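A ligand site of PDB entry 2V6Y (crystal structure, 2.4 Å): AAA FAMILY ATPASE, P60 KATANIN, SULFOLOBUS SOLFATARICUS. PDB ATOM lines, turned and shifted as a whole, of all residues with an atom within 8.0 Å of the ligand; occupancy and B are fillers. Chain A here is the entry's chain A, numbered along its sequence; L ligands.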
ATOM      1  N   SER A   2       4.540 -30.868 -11.870  1.00  0.00           N
ATOM      2  CA  SER A   2       5.153 -29.561 -11.691  1.00  0.00           C
ATOM      3  C   SER A   2       5.420 -29.334 -10.201  1.00  0.00           C
ATOM      4  O   SER A   2       4.762 -29.917  -9.359  1.00  0.00           O
ATOM      5  CB  SER A   2       4.256 -28.446 -12.235  1.00  0.00           C
ATOM      6  OG  SER A   2       3.335 -27.995 -11.262  1.00  0.00           O
ATOM      7  N   ALA A   3       6.401 -28.494  -9.902  1.00  0.00           N
ATOM      8  CA  ALA A   3       6.848 -28.246  -8.550  1.00  0.00           C
ATOM      9  C   ALA A   3       5.730 -27.630  -7.712  1.00  0.00           C
ATOM     10  O   ALA A   3       5.620 -27.912  -6.512  1.00  0.00           O
ATOM     11  CB  ALA A   3       8.042 -27.323  -8.556  1.00  0.00           C
ATOM     12  N   GLN A   4       4.900 -26.786  -8.339  1.00  0.00           N
ATOM     13  CA  GLN A   4       3.820 -26.085  -7.636  1.00  0.00           C
ATOM     14  C   GLN A   4       2.740 -27.059  -7.167  1.00  0.00           C
ATOM     15  O   GLN A   4       2.274 -26.964  -6.033  1.00  0.00           O
ATOM     16  CB  GLN A   4       3.198 -25.004  -8.520  1.00  0.00           C
ATOM     17  CG  GLN A   4       2.011 -24.281  -7.887  1.00  0.00           C
ATOM     18  CD  GLN A   4       1.522 -23.100  -8.704  1.00  0.00           C
ATOM     19  OE1 GLN A   4       1.625 -23.092  -9.934  1.00  0.00           O
ATOM     20  NE2 GLN A   4       0.987 -22.094  -8.025  1.00  0.00           N
ATOM     21  N   VAL A   5       2.342 -27.978  -8.030  1.00  0.00           N
ATOM     22  CA  VAL A   5       1.293 -28.946  -7.714  1.00  0.00           C
ATOM     23  C   VAL A   5       1.760 -29.956  -6.656  1.00  0.00           C
ATOM     24  O   VAL A   5       1.013 -30.269  -5.741  1.00  0.00           O
ATOM     25  CB  VAL A   5       0.744 -29.645  -9.001  1.00  0.00           C
ATOM     26  CG1 VAL A   5      -0.306 -30.692  -8.667  1.00  0.00           C
ATOM     27  CG2 VAL A   5       0.158 -28.607  -9.957  1.00  0.00           C
ATOM     28  N   GLU A   8       1.706 -28.037  -3.384  1.00  0.00           N
ATOM     29  CA  GLU A   8       0.303 -27.906  -2.985  1.00  0.00           C
ATOM     30  C   GLU A   8      -0.224 -29.184  -2.364  1.00  0.00           C
ATOM     31  O   GLU A   8      -0.958 -29.123  -1.378  1.00  0.00           O
ATOM     32  CB  GLU A   8      -0.578 -27.560  -4.178  1.00  0.00           C
ATOM     33  CG  GLU A   8      -0.601 -26.102  -4.507  1.00  0.00           C
ATOM     34  CD  GLU A   8      -1.329 -25.818  -5.802  1.00  0.00           C
ATOM     35  OE1 GLU A   8      -1.955 -26.731  -6.399  1.00  0.00           O
ATOM     36  OE2 GLU A   8      -1.287 -24.639  -6.229  1.00  0.00           O
ATOM     37  N   ILE A  44       5.714 -22.100  -1.647  1.00  0.00           N
ATOM     38  CA  ILE A  44       5.048 -21.906  -2.937  1.00  0.00           C
ATOM     39  C   ILE A  44       4.970 -20.421  -3.292  1.00  0.00           C
ATOM     40  O   ILE A  44       5.167 -20.063  -4.442  1.00  0.00           O
ATOM     41  CB  ILE A  44       3.581 -22.508  -2.978  1.00  0.00           C
ATOM     42  CG1 ILE A  44       3.531 -23.971  -2.530  1.00  0.00           C
ATOM     43  CG2 ILE A  44       2.959 -22.386  -4.387  1.00  0.00           C
ATOM     44  CD1 ILE A  44       2.080 -24.457  -2.224  1.00  0.00           C
ATOM     45  N   LEU A  47       8.328 -19.356  -4.427  1.00  0.00           N
ATOM     46  CA  LEU A  47       8.677 -19.847  -5.765  1.00  0.00           C
ATOM     47  C   LEU A  47       7.766 -19.309  -6.873  1.00  0.00           C
ATOM     48  O   LEU A  47       8.205 -19.130  -8.020  1.00  0.00           O
ATOM     49  CB  LEU A  47       8.674 -21.378  -5.823  1.00  0.00           C
ATOM     50  CG  LEU A  47       9.656 -22.151  -4.944  1.00  0.00           C
ATOM     51  CD1 LEU A  47       9.488 -23.645  -5.221  1.00  0.00           C
ATOM     52  CD2 LEU A  47      11.116 -21.702  -5.182  1.00  0.00           C
ATOM     53  N   TYR A  48       6.493 -19.091  -6.517  1.00  0.00           N
ATOM     54  CA  TYR A  48       5.482 -18.612  -7.445  1.00  0.00           C
ATOM     55  C   TYR A  48       4.767 -17.403  -6.844  1.00  0.00           C
ATOM     56  O   TYR A  48       3.588 -17.488  -6.513  1.00  0.00           O
ATOM     57  CB  TYR A  48       4.485 -19.730  -7.796  1.00  0.00           C
ATOM     58  CG  TYR A  48       5.184 -20.923  -8.391  1.00  0.00           C
ATOM     59  CD1 TYR A  48       5.537 -20.946  -9.741  1.00  0.00           C
ATOM     60  CD2 TYR A  48       5.566 -22.008  -7.583  1.00  0.00           C
ATOM     61  CE1 TYR A  48       6.203 -22.023 -10.310  1.00  0.00           C
ATOM     62  CE2 TYR A  48       6.264 -23.098  -8.143  1.00  0.00           C
ATOM     63  CZ  TYR A  48       6.568 -23.091  -9.496  1.00  0.00           C
ATOM     64  OH  TYR A  48       7.249 -24.166 -10.049  1.00  0.00           O
ATOM     65  N   PRO A  49       5.497 -16.273  -6.715  1.00  0.00           N
ATOM     66  CA  PRO A  49       4.896 -15.129  -6.056  1.00  0.00           C
ATOM     67  C   PRO A  49       3.755 -14.491  -6.866  1.00  0.00           C
ATOM     68  O   PRO A  49       2.899 -13.845  -6.276  1.00  0.00           O
ATOM     69  CB  PRO A  49       6.081 -14.171  -5.879  1.00  0.00           C
ATOM     70  CG  PRO A  49       7.083 -14.550  -6.932  1.00  0.00           C
ATOM     71  CD  PRO A  49       6.864 -16.001  -7.218  1.00  0.00           C
ATOM     72  N   GLU A  50       3.711 -14.694  -8.178  1.00  0.00           N
ATOM     73  CA  GLU A  50       2.570 -14.177  -8.925  1.00  0.00           C
ATOM     74  C   GLU A  50       1.598 -15.252  -9.447  1.00  0.00           C
ATOM     75  O   GLU A  50       0.972 -15.096 -10.492  1.00  0.00           O
ATOM     76  CB  GLU A  50       2.976 -13.143  -9.982  1.00  0.00           C
ATOM     77  CG  GLU A  50       3.867 -13.602 -11.083  1.00  0.00           C
ATOM     78  CD  GLU A  50       4.389 -12.437 -11.914  1.00  0.00           C
ATOM     79  OE1 GLU A  50       4.214 -11.258 -11.515  1.00  0.00           O
ATOM     80  OE2 GLU A  50       4.999 -12.709 -12.972  1.00  0.00           O
ATOM     81  N   SER A  51       1.468 -16.328  -8.680  1.00  0.00           N
ATOM     82  CA  SER A  51       0.486 -17.371  -8.941  1.00  0.00           C
ATOM     83  C   SER A  51      -0.895 -16.783  -8.719  1.00  0.00           C
ATOM     84  O   SER A  51      -1.086 -16.022  -7.771  1.00  0.00           O
ATOM     85  CB  SER A  51       0.715 -18.561  -8.003  1.00  0.00           C
ATOM     86  OG  SER A  51      -0.437 -19.376  -7.898  1.00  0.00           O
ATOM     87  N   VAL A  52      -1.853 -17.130  -9.578  1.00  0.00           N
ATOM     88  CA  VAL A  52      -3.265 -16.742  -9.386  1.00  0.00           C
ATOM     89  C   VAL A  52      -3.843 -17.227  -8.052  1.00  0.00           C
ATOM     90  O   VAL A  52      -4.862 -16.718  -7.617  1.00  0.00           O
ATOM     91  CB  VAL A  52      -4.200 -17.194 -10.551  1.00  0.00           C
ATOM     92  CG1 VAL A  52      -3.814 -16.512 -11.850  1.00  0.00           C
ATOM     93  CG2 VAL A  52      -4.223 -18.735 -10.691  1.00  0.00           C
ATOM     94  N   ALA A  53      -3.190 -18.189  -7.415  1.00  0.00           N
ATOM     95  CA  ALA A  53      -3.678 -18.777  -6.183  1.00  0.00           C
ATOM     96  C   ALA A  53      -2.929 -18.241  -4.961  1.00  0.00           C
ATOM     97  O   ALA A  53      -2.989 -18.804  -3.876  1.00  0.00           O
ATOM     98  CB  ALA A  53      -3.559 -20.289  -6.243  1.00  0.00           C
ATOM     99  N   ARG A  54      -2.207 -17.147  -5.162  1.00  0.00           N
ATOM    100  CA  ARG A  54      -1.430 -16.539  -4.100  1.00  0.00           C
ATOM    101  C   ARG A  54      -2.269 -15.992  -2.930  1.00  0.00           C
ATOM    102  O   ARG A  54      -1.880 -16.143  -1.774  1.00  0.00           O
ATOM    103  CB  ARG A  54      -0.505 -15.455  -4.669  1.00  0.00           C
ATOM    104  CG  ARG A  54      -0.058 -14.456  -3.632  1.00  0.00           C
ATOM    105  CD  ARG A  54       1.407 -14.330  -3.652  1.00  0.00           C
ATOM    106  NE  ARG A  54       1.855 -13.296  -2.746  1.00  0.00           N
ATOM    107  CZ  ARG A  54       2.867 -12.480  -2.985  1.00  0.00           C
ATOM    108  NH1 ARG A  54       3.526 -12.551  -4.119  1.00  0.00           N
ATOM    109  NH2 ARG A  54       3.223 -11.583  -2.089  1.00  0.00           N
ATOM    110  N   TYR A  57      -3.387 -19.055  -0.905  1.00  0.00           N
ATOM    111  CA  TYR A  57      -2.359 -19.618  -0.029  1.00  0.00           C
ATOM    112  C   TYR A  57      -2.205 -18.736   1.198  1.00  0.00           C
ATOM    113  O   TYR A  57      -2.001 -19.208   2.303  1.00  0.00           O
ATOM    114  CB  TYR A  57      -1.000 -19.733  -0.719  1.00  0.00           C
ATOM    115  CG  TYR A  57      -0.932 -20.515  -2.010  1.00  0.00           C
ATOM    116  CD1 TYR A  57      -1.654 -21.693  -2.194  1.00  0.00           C
ATOM    117  CD2 TYR A  57      -0.071 -20.111  -3.020  1.00  0.00           C
ATOM    118  CE1 TYR A  57      -1.566 -22.423  -3.397  1.00  0.00           C
ATOM    119  CE2 TYR A  57       0.029 -20.806  -4.202  1.00  0.00           C
ATOM    120  CZ  TYR A  57      -0.721 -21.960  -4.394  1.00  0.00           C
ATOM    121  OH  TYR A  57      -0.571 -22.629  -5.588  1.00  0.00           O
HETATM  122  O1  LIG L   1       3.817 -21.821 -12.686  1.00  0.00           O
HETATM  123  O2  LIG L   1       2.580 -20.839 -14.236  1.00  0.00           O
HETATM  124  C1  LIG L   1       2.822 -21.117 -13.029  1.00  0.00           C
HETATM  125  C2  LIG L   1       1.910 -20.582 -11.943  1.00  0.00           C
HETATM  126  O3  LIG L   1       2.336 -19.242 -11.664  1.00  0.00           O
HETATM  127  C3  LIG L   1       0.419 -20.639 -12.364  1.00  0.00           C
HETATM  128  O4  LIG L   1      -0.029 -22.016 -12.392  1.00  0.00           O
HETATM  129  C4  LIG L   1      -0.507 -19.850 -11.457  1.00  0.00           C
HETATM  130  O5  LIG L   1      -0.891 -20.344 -10.364  1.00  0.00           O
HETATM  131  O6  LIG L   1      -0.874 -18.715 -11.853  1.00  0.00           O
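An oxygen (O5) of the ligand lies within hydrogen-bond range of the side-chain hydroxyl of Ser 51.
The backbone NH (N) of Val 52 lies within hydrogen-bond range of an oxygen (O6) of the ligand (2.9 Å).
OE1 of Gln 4 is in hydrogen-bond range of O4 of the ligand (3.2 Å).
The side-chain amide nitrogen (NE2) of Gln 4 sits at hydrogen-bond distance from the side-chain hydroxyl (OG) of Ser 51, 3.1 Å away.
The side-chain hydroxyl of Ser 51 lies close to the backbone NH of Ala 53, at 3.0 Å.
OH of Tyr 57 is in hydrogen-bond range of NE2 of Gln 4 (2.9 Å).
CE1 of Tyr 48 touches O1 of the ligand (3.4 Å).
Within 4 Å of the ligand: Gln 4, Tyr 48, Ser 51 and Val 52.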
